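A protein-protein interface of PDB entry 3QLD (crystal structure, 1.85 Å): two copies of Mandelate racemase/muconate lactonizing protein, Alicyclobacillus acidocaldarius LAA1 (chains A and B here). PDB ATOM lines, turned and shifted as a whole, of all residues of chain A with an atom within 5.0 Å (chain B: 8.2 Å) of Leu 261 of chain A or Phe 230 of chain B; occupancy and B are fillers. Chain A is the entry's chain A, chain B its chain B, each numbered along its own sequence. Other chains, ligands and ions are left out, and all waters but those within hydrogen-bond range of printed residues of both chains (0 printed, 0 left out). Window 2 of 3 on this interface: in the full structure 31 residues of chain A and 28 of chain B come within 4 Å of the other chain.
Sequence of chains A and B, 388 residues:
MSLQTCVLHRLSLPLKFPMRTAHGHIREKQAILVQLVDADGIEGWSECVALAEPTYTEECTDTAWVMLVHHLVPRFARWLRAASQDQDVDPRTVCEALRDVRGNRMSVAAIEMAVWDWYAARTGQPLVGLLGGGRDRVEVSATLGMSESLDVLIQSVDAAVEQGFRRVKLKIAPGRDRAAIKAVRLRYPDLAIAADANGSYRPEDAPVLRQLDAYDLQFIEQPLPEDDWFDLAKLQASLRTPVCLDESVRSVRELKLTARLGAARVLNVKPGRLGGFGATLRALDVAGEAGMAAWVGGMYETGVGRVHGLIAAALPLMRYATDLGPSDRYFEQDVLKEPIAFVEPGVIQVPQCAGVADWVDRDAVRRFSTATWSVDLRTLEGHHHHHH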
ATOM      1  N   TRP A 229     -10.528  -3.983   8.359  1.00  0.00           N
ATOM      2  CA  TRP A 229      -9.673  -3.955   7.230  1.00  0.00           C
ATOM      3  C   TRP A 229      -9.853  -2.657   6.453  1.00  0.00           C
ATOM      4  O   TRP A 229      -8.890  -2.112   5.895  1.00  0.00           O
ATOM      5  CB  TRP A 229     -10.024  -5.137   6.344  1.00  0.00           C
ATOM      6  CG  TRP A 229      -9.423  -6.434   6.767  1.00  0.00           C
ATOM      7  CD1 TRP A 229     -10.088  -7.539   7.252  1.00  0.00           C
ATOM      8  CD2 TRP A 229      -8.030  -6.772   6.770  1.00  0.00           C
ATOM      9  NE1 TRP A 229      -9.181  -8.554   7.529  1.00  0.00           N
ATOM     10  CE2 TRP A 229      -7.917  -8.109   7.240  1.00  0.00           C
ATOM     11  CE3 TRP A 229      -6.859  -6.073   6.403  1.00  0.00           C
ATOM     12  CZ2 TRP A 229      -6.681  -8.765   7.358  1.00  0.00           C
ATOM     13  CZ3 TRP A 229      -5.623  -6.745   6.483  1.00  0.00           C
ATOM     14  CH2 TRP A 229      -5.547  -8.066   6.972  1.00  0.00           C
ATOM     15  N   PHE A 230     -11.086  -2.134   6.437  1.00  0.00           N
ATOM     16  CA  PHE A 230     -11.312  -0.920   5.690  1.00  0.00           C
ATOM     17  C   PHE A 230     -10.794   0.309   6.373  1.00  0.00           C
ATOM     18  O   PHE A 230     -10.357   1.214   5.678  1.00  0.00           O
ATOM     19  CB  PHE A 230     -12.768  -0.777   5.230  1.00  0.00           C
ATOM     20  CG  PHE A 230     -12.953  -1.351   3.872  1.00  0.00           C
ATOM     21  CD1 PHE A 230     -13.523  -2.593   3.705  1.00  0.00           C
ATOM     22  CD2 PHE A 230     -12.395  -0.703   2.757  1.00  0.00           C
ATOM     23  CE1 PHE A 230     -13.629  -3.146   2.433  1.00  0.00           C
ATOM     24  CE2 PHE A 230     -12.495  -1.224   1.489  1.00  0.00           C
ATOM     25  CZ  PHE A 230     -13.118  -2.459   1.317  1.00  0.00           C
ATOM     26  N   ALA A 233      -7.174   0.233   5.359  1.00  0.00           N
ATOM     27  CA  ALA A 233      -7.031   0.636   3.970  1.00  0.00           C
ATOM     28  C   ALA A 233      -7.122   2.134   3.848  1.00  0.00           C
ATOM     29  O   ALA A 233      -6.318   2.771   3.119  1.00  0.00           O
ATOM     30  CB  ALA A 233      -8.127  -0.041   3.093  1.00  0.00           C
ATOM     31  N   LEU A 257      -5.151 -10.277   0.614  1.00  0.00           N
ATOM     32  CA  LEU A 257      -6.210  -9.331   0.926  1.00  0.00           C
ATOM     33  C   LEU A 257      -5.569  -7.961   1.292  1.00  0.00           C
ATOM     34  O   LEU A 257      -6.038  -6.891   0.854  1.00  0.00           O
ATOM     35  CB  LEU A 257      -7.069  -9.860   2.101  1.00  0.00           C
ATOM     36  CG  LEU A 257      -8.069  -8.818   2.652  1.00  0.00           C
ATOM     37  CD1 LEU A 257      -9.150  -8.402   1.575  1.00  0.00           C
ATOM     38  CD2 LEU A 257      -8.716  -9.255   3.942  1.00  0.00           C
ATOM     39  N   THR A 258      -4.520  -7.998   2.121  1.00  0.00           N
ATOM     40  CA  THR A 258      -3.759  -6.756   2.456  1.00  0.00           C
ATOM     41  C   THR A 258      -3.358  -5.964   1.236  1.00  0.00           C
ATOM     42  O   THR A 258      -3.638  -4.755   1.136  1.00  0.00           O
ATOM     43  CB  THR A 258      -2.500  -7.089   3.277  1.00  0.00           C
ATOM     44  OG1 THR A 258      -2.931  -7.632   4.506  1.00  0.00           O
ATOM     45  CG2 THR A 258      -1.704  -5.823   3.590  1.00  0.00           C
ATOM     46  N   ALA A 259      -2.747  -6.683   0.296  1.00  0.00           N
ATOM     47  CA  ALA A 259      -2.267  -6.113  -0.950  1.00  0.00           C
ATOM     48  C   ALA A 259      -3.434  -5.606  -1.802  1.00  0.00           C
ATOM     49  O   ALA A 259      -3.332  -4.555  -2.413  1.00  0.00           O
ATOM     50  CB  ALA A 259      -1.449  -7.149  -1.696  1.00  0.00           C
ATOM     51  N   ARG A 260      -4.552  -6.334  -1.814  1.00  0.00           N
ATOM     52  CA  ARG A 260      -5.705  -5.966  -2.614  1.00  0.00           C
ATOM     53  C   ARG A 260      -6.342  -4.672  -2.079  1.00  0.00           C
ATOM     54  O   ARG A 260      -6.778  -3.801  -2.864  1.00  0.00           O
ATOM     55  CB  ARG A 260      -6.716  -7.132  -2.682  1.00  0.00           C
ATOM     56  CG  ARG A 260      -7.935  -6.872  -3.559  1.00  0.00           C
ATOM     57  CD  ARG A 260      -7.622  -6.928  -5.048  1.00  0.00           C
ATOM     58  NE  ARG A 260      -8.829  -6.658  -5.816  1.00  0.00           N
ATOM     59  CZ  ARG A 260      -9.544  -7.587  -6.479  1.00  0.00           C
ATOM     60  NH1 ARG A 260      -9.164  -8.860  -6.495  1.00  0.00           N
ATOM     61  NH2 ARG A 260     -10.641  -7.235  -7.161  1.00  0.00           N
ATOM     62  N   LEU A 261      -6.316  -4.524  -0.740  1.00  0.00           N
ATOM     63  CA  LEU A 261      -6.918  -3.389  -0.067  1.00  0.00           C
ATOM     64  C   LEU A 261      -6.006  -2.172  -0.067  1.00  0.00           C
ATOM     65  O   LEU A 261      -6.490  -1.083   0.163  1.00  0.00           O
ATOM     66  CB  LEU A 261      -7.265  -3.744   1.380  1.00  0.00           C
ATOM     67  CG  LEU A 261      -8.511  -4.589   1.597  1.00  0.00           C
ATOM     68  CD1 LEU A 261      -8.508  -4.963   3.062  1.00  0.00           C
ATOM     69  CD2 LEU A 261      -9.830  -3.910   1.156  1.00  0.00           C
ATOM     70  N   GLY A 262      -4.708  -2.375  -0.340  1.00  0.00           N
ATOM     71  CA  GLY A 262      -3.700  -1.302  -0.202  1.00  0.00           C
ATOM     72  C   GLY A 262      -3.605  -0.973   1.292  1.00  0.00           C
ATOM     73  O   GLY A 262      -3.504   0.196   1.667  1.00  0.00           O
ATOM     74  N   ALA A 263      -3.728  -1.993   2.140  1.00  0.00           N
ATOM     75  CA  ALA A 263      -3.847  -1.741   3.574  1.00  0.00           C
ATOM     76  C   ALA A 263      -2.467  -1.593   4.214  1.00  0.00           C
ATOM     77  O   ALA A 263      -2.351  -1.140   5.391  1.00  0.00           O
ATOM     78  CB  ALA A 263      -4.567  -2.883   4.268  1.00  0.00           C
ATOM     79  N   PRO B 203     -15.103 -18.133  -9.515  1.00  0.00           N
ATOM     80  CA  PRO B 203     -15.809 -16.952 -10.076  1.00  0.00           C
ATOM     81  C   PRO B 203     -16.440 -17.176 -11.500  1.00  0.00           C
ATOM     82  O   PRO B 203     -17.558 -16.660 -11.806  1.00  0.00           O
ATOM     83  CB  PRO B 203     -14.702 -15.886 -10.144  1.00  0.00           C
ATOM     84  CG  PRO B 203     -13.632 -16.373  -9.167  1.00  0.00           C
ATOM     85  CD  PRO B 203     -13.729 -17.836  -9.031  1.00  0.00           C
ATOM     86  N   LEU B 224     -17.753 -19.898  -2.849  1.00  0.00           N
ATOM     87  CA  LEU B 224     -16.345 -19.737  -3.262  1.00  0.00           C
ATOM     88  C   LEU B 224     -15.414 -20.124  -2.126  1.00  0.00           C
ATOM     89  O   LEU B 224     -15.871 -20.296  -0.971  1.00  0.00           O
ATOM     90  CB  LEU B 224     -16.107 -18.265  -3.678  1.00  0.00           C
ATOM     91  CG  LEU B 224     -17.004 -17.758  -4.825  1.00  0.00           C
ATOM     92  CD1 LEU B 224     -16.716 -16.257  -5.135  1.00  0.00           C
ATOM     93  CD2 LEU B 224     -16.738 -18.616  -6.088  1.00  0.00           C
ATOM     94  N   ASP B 227     -12.248 -16.496   1.983  1.00  0.00           N
ATOM     95  CA  ASP B 227     -11.360 -15.313   1.734  1.00  0.00           C
ATOM     96  C   ASP B 227     -11.186 -14.893   0.275  1.00  0.00           C
ATOM     97  O   ASP B 227     -10.350 -14.039   0.013  1.00  0.00           O
ATOM     98  CB  ASP B 227      -9.917 -15.482   2.286  1.00  0.00           C
ATOM     99  CG  ASP B 227      -9.852 -15.995   3.731  1.00  0.00           C
ATOM    100  OD1 ASP B 227     -10.619 -15.531   4.623  1.00  0.00           O
ATOM    101  OD2 ASP B 227      -8.985 -16.873   3.956  1.00  0.00           O
ATOM    102  N   ASP B 228     -11.909 -15.474  -0.682  1.00  0.00           N
ATOM    103  CA  ASP B 228     -12.000 -14.882  -2.006  1.00  0.00           C
ATOM    104  C   ASP B 228     -12.924 -13.648  -1.858  1.00  0.00           C
ATOM    105  O   ASP B 228     -13.926 -13.579  -2.538  1.00  0.00           O
ATOM    106  CB  ASP B 228     -12.703 -15.857  -2.956  1.00  0.00           C
ATOM    107  CG  ASP B 228     -11.775 -16.600  -3.894  1.00  0.00           C
ATOM    108  OD1 ASP B 228     -10.641 -16.934  -3.482  1.00  0.00           O
ATOM    109  OD2 ASP B 228     -12.244 -16.895  -5.045  1.00  0.00           O
ATOM    110  N   TRP B 229     -12.609 -12.685  -0.992  1.00  0.00           N
ATOM    111  CA  TRP B 229     -13.577 -11.589  -0.656  1.00  0.00           C
ATOM    112  C   TRP B 229     -14.043 -10.731  -1.830  1.00  0.00           C
ATOM    113  O   TRP B 229     -15.251 -10.518  -1.996  1.00  0.00           O
ATOM    114  CB  TRP B 229     -12.991 -10.674   0.418  1.00  0.00           C
ATOM    115  CG  TRP B 229     -12.892 -11.355   1.724  1.00  0.00           C
ATOM    116  CD1 TRP B 229     -11.751 -11.857   2.323  1.00  0.00           C
ATOM    117  CD2 TRP B 229     -13.973 -11.665   2.592  1.00  0.00           C
ATOM    118  NE1 TRP B 229     -12.068 -12.424   3.527  1.00  0.00           N
ATOM    119  CE2 TRP B 229     -13.425 -12.330   3.714  1.00  0.00           C
ATOM    120  CE3 TRP B 229     -15.366 -11.450   2.534  1.00  0.00           C
ATOM    121  CZ2 TRP B 229     -14.208 -12.792   4.751  1.00  0.00           C
ATOM    122  CZ3 TRP B 229     -16.145 -11.914   3.599  1.00  0.00           C
ATOM    123  CH2 TRP B 229     -15.547 -12.574   4.680  1.00  0.00           C
ATOM    124  N   PHE B 230     -13.096 -10.249  -2.643  1.00  0.00           N
ATOM    125  CA  PHE B 230     -13.465  -9.450  -3.813  1.00  0.00           C
ATOM    126  C   PHE B 230     -14.222 -10.240  -4.840  1.00  0.00           C
ATOM    127  O   PHE B 230     -15.227  -9.773  -5.332  1.00  0.00           O
ATOM    128  CB  PHE B 230     -12.249  -8.700  -4.398  1.00  0.00           C
ATOM    129  CG  PHE B 230     -11.910  -7.502  -3.631  1.00  0.00           C
ATOM    130  CD1 PHE B 230     -11.410  -7.620  -2.341  1.00  0.00           C
ATOM    131  CD2 PHE B 230     -12.130  -6.224  -4.179  1.00  0.00           C
ATOM    132  CE1 PHE B 230     -11.093  -6.466  -1.544  1.00  0.00           C
ATOM    133  CE2 PHE B 230     -11.834  -5.060  -3.412  1.00  0.00           C
ATOM    134  CZ  PHE B 230     -11.335  -5.183  -2.075  1.00  0.00           C
ATOM    135  N   ASP B 231     -13.785 -11.463  -5.135  1.00  0.00           N
ATOM    136  CA  ASP B 231     -14.585 -12.354  -6.012  1.00  0.00           C
ATOM    137  C   ASP B 231     -16.030 -12.618  -5.492  1.00  0.00           C
ATOM    138  O   ASP B 231     -16.996 -12.657  -6.248  1.00  0.00           O
ATOM    139  CB  ASP B 231     -13.841 -13.677  -6.257  1.00  0.00           C
ATOM    140  CG  ASP B 231     -12.563 -13.488  -7.052  1.00  0.00           C
ATOM    141  OD1 ASP B 231     -12.549 -12.662  -8.006  1.00  0.00           O
ATOM    142  OD2 ASP B 231     -11.603 -14.214  -6.749  1.00  0.00           O
ATOM    143  N   LEU B 232     -16.156 -12.761  -4.181  1.00  0.00           N
ATOM    144  CA  LEU B 232     -17.456 -12.982  -3.567  1.00  0.00           C
ATOM    145  C   LEU B 232     -18.354 -11.790  -3.716  1.00  0.00           C
ATOM    146  O   LEU B 232     -19.504 -11.927  -4.043  1.00  0.00           O
ATOM    147  CB  LEU B 232     -17.225 -13.270  -2.095  1.00  0.00           C
ATOM    148  CG  LEU B 232     -18.423 -13.907  -1.430  1.00  0.00           C
ATOM    149  CD1 LEU B 232     -18.838 -15.261  -2.103  1.00  0.00           C
ATOM    150  CD2 LEU B 232     -18.063 -14.125  -0.010  1.00  0.00           C
ATOM    151  N   ALA B 233     -17.806 -10.579  -3.525  1.00  0.00           N
ATOM    152  CA  ALA B 233     -18.612  -9.383  -3.605  1.00  0.00           C
ATOM    153  C   ALA B 233     -19.108  -9.269  -5.073  1.00  0.00           C
ATOM    154  O   ALA B 233     -20.286  -9.002  -5.319  1.00  0.00           O
ATOM    155  CB  ALA B 233     -17.791  -8.203  -3.194  1.00  0.00           C
ATOM    156  N   LYS B 234     -18.236  -9.579  -6.034  1.00  0.00           N
ATOM    157  CA  LYS B 234     -18.675  -9.508  -7.437  1.00  0.00           C
ATOM    158  C   LYS B 234     -19.717 -10.556  -7.746  1.00  0.00           C
ATOM    159  O   LYS B 234     -20.666 -10.297  -8.455  1.00  0.00           O
ATOM    160  CB  LYS B 234     -17.476  -9.617  -8.403  1.00  0.00           C
ATOM    161  CG  LYS B 234     -16.569  -8.382  -8.269  1.00  0.00           C
ATOM    162  CD  LYS B 234     -15.302  -8.460  -9.179  1.00  0.00           C
ATOM    163  CE  LYS B 234     -14.202  -7.484  -8.710  1.00  0.00           C
ATOM    164  NZ  LYS B 234     -12.937  -7.768  -9.497  1.00  0.00           N
ATOM    165  N   LEU B 235     -19.537 -11.765  -7.204  1.00  0.00           N
ATOM    166  CA  LEU B 235     -20.524 -12.808  -7.433  1.00  0.00           C
ATOM    167  C   LEU B 235     -21.867 -12.471  -6.839  1.00  0.00           C
ATOM    168  O   LEU B 235     -22.905 -12.635  -7.490  1.00  0.00           O
ATOM    169  CB  LEU B 235     -20.055 -14.186  -6.909  1.00  0.00           C
ATOM    170  CG  LEU B 235     -21.116 -15.326  -6.885  1.00  0.00           C
ATOM    171  CD1 LEU B 235     -21.485 -15.762  -8.279  1.00  0.00           C
ATOM    172  CD2 LEU B 235     -20.523 -16.529  -6.094  1.00  0.00           C
ATOM    173  N   GLN B 236     -21.885 -11.955  -5.607  1.00  0.00           N
ATOM    174  CA  GLN B 236     -23.198 -11.660  -4.995  1.00  0.00           C
ATOM    175  C   GLN B 236     -23.927 -10.550  -5.734  1.00  0.00           C
ATOM    176  O   GLN B 236     -25.156 -10.550  -5.793  1.00  0.00           O
ATOM    177  CB  GLN B 236     -23.002 -11.294  -3.510  1.00  0.00           C
ATOM    178  CG  GLN B 236     -24.253 -10.752  -2.784  1.00  0.00           C
ATOM    179  CD  GLN B 236     -25.290 -11.834  -2.509  1.00  0.00           C
ATOM    180  OE1 GLN B 236     -25.367 -12.381  -1.397  1.00  0.00           O
ATOM    181  NE2 GLN B 236     -26.019 -12.198  -3.526  1.00  0.00           N
ATOM    182  N   ALA B 237     -23.162  -9.590  -6.268  1.00  0.00           N
ATOM    183  CA  ALA B 237     -23.725  -8.481  -7.028  1.00  0.00           C
ATOM    184  C   ALA B 237     -24.509  -8.939  -8.260  1.00  0.00           C
ATOM    185  O   ALA B 237     -25.516  -8.324  -8.635  1.00  0.00           O
ATOM    186  CB  ALA B 237     -22.608  -7.497  -7.427  1.00  0.00           C
ATOM    187  N   LEU B 257     -16.185  -6.386   7.107  1.00  0.00           N
ATOM    188  CA  LEU B 257     -15.641  -6.584   5.782  1.00  0.00           C
ATOM    189  C   LEU B 257     -16.704  -7.062   4.822  1.00  0.00           C
ATOM    190  O   LEU B 257     -16.854  -6.485   3.767  1.00  0.00           O
ATOM    191  CB  LEU B 257     -14.516  -7.619   5.828  1.00  0.00           C
ATOM    192  CG  LEU B 257     -13.819  -7.872   4.498  1.00  0.00           C
ATOM    193  CD1 LEU B 257     -13.140  -6.594   4.037  1.00  0.00           C
ATOM    194  CD2 LEU B 257     -12.803  -8.963   4.644  1.00  0.00           C
ATOM    195  N   ARG B 260     -19.192  -4.102   4.165  1.00  0.00           N
ATOM    196  CA  ARG B 260     -18.621  -3.008   3.325  1.00  0.00           C
ATOM    197  C   ARG B 260     -18.474  -3.346   1.844  1.00  0.00           C
ATOM    198  O   ARG B 260     -18.582  -2.486   0.975  1.00  0.00           O
ATOM    199  CB  ARG B 260     -17.229  -2.622   3.847  1.00  0.00           C
ATOM    200  CG  ARG B 260     -17.167  -2.000   5.228  1.00  0.00           C
ATOM    201  CD  ARG B 260     -17.819  -0.597   5.280  1.00  0.00           C
ATOM    202  NE  ARG B 260     -16.962   0.445   4.716  1.00  0.00           N
ATOM    203  CZ  ARG B 260     -16.003   1.096   5.379  1.00  0.00           C
ATOM    204  NH1 ARG B 260     -15.726   0.810   6.645  1.00  0.00           N
ATOM    205  NH2 ARG B 260     -15.301   2.035   4.764  1.00  0.00           N
ATOM    206  N   LEU B 261     -18.189  -4.614   1.564  1.00  0.00           N
ATOM    207  CA  LEU B 261     -18.102  -5.111   0.204  1.00  0.00           C
ATOM    208  C   LEU B 261     -19.436  -5.623  -0.379  1.00  0.00           C
ATOM    209  O   LEU B 261     -19.488  -5.931  -1.566  1.00  0.00           O
ATOM    210  CB  LEU B 261     -17.104  -6.267   0.143  1.00  0.00           C
ATOM    211  CG  LEU B 261     -15.627  -5.897   0.198  1.00  0.00           C
ATOM    212  CD1 LEU B 261     -14.858  -7.217   0.252  1.00  0.00           C
ATOM    213  CD2 LEU B 261     -15.232  -5.075  -1.021  1.00  0.00           C
ATOM    214  N   GLY B 262     -20.469  -5.752   0.443  1.00  0.00           N
ATOM    215  CA  GLY B 262     -21.719  -6.396  -0.008  1.00  0.00           C
ATOM    216  C   GLY B 262     -21.500  -7.850  -0.446  1.00  0.00           C
ATOM    217  O   GLY B 262     -22.130  -8.323  -1.393  1.00  0.00           O
ATOM    218  N   ALA B 263     -20.619  -8.556   0.256  1.00  0.00           N
ATOM    219  CA  ALA B 263     -20.180  -9.890  -0.193  1.00  0.00           C
ATOM    220  C   ALA B 263     -21.166 -11.001   0.147  1.00  0.00           C
ATOM    221  O   ALA B 263     -21.091 -12.096  -0.447  1.00  0.00           O
ATOM    222  CB  ALA B 263     -18.833 -10.227   0.376  1.00  0.00           C
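Among the printed residues, pairs that only touch across the chains: Arg 260 of chain A with Phe 230 of chain B (3.5 Å), Phe 230 of chain A with Arg 260 of chain B (3.6 Å), Leu 261 of chain A with Phe 230 of chain B (3.8 Å) and Phe 230 of chain A with Leu 257 of chain B (3.8 Å).
Leu 261 of chain A touches one residue of chain B. Of chain A, only Arg 260 and Leu 261 come within 4 Å of Phe 230 of chain B. No residue of chain B comes within 4 Å of Gly 262 of chain A. Of the printed residues of chain B, Arg 260 of chain A touches Phe 230 and Lys 234. Of the printed residues of chain B, Phe 230 of chain A touches Leu 257 and Arg 260. Of the printed residues of chain A, Lys 234 of chain B touches Arg 260 (3.3 Å). Leu 235 of chain B touches none of the printed residues of chain A. Ala 233 of chain A touches none of the printed residues of chain B. The nearest residue of chain B that does not touch Leu 261 of chain A is Leu 257 of chain B (5.0 Å). The nearest printed residue of chain A that does not touch Lys 234 of chain B is Phe 230 of chain A (11.3 Å).
Phe 230 of chain A touches Leu 257 of chain B, but with the chains exchanged Leu 257 of chain A does not touch Phe 230 of chain B (4.2 Å). Phe 230 of chain A touches Arg 260 of chain B, and with the chains exchanged Arg 260 of chain A touches Phe 230 of chain B. Leu 261 of chain A touches Phe 230 of chain B, but with the chains exchanged Phe 230 of chain A does not touch Leu 261 of chain B (4.1 Å). Positions printed for both chains: 229, 230, 233, 257, 260, 261, 262 and 263. Of the 5 pairs that touch across the chains among the printed residues, 2 have their exchanged pair printed and touching as well.
Of the 18 printed residues of chain B, 4 touch a printed residue of chain A. Printed residues of chain A that touch a printed residue of chain B: Phe 230, Arg 260 and Leu 261. Hydrophobic or aromatic side chains of chain A within 4 Å of the printed part of chain B: Phe 230 and Leu 261. Among the printed residues, no Asp or Glu carboxylate lies within 4 Å of a Lys or Arg side-chain nitrogen of the other chain.
The guanidinium group (NH2) of Arg 260 of chain A sits close to the side-chain amino group (NZ) of Lys 234 of chain B, 3.3 Å away.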
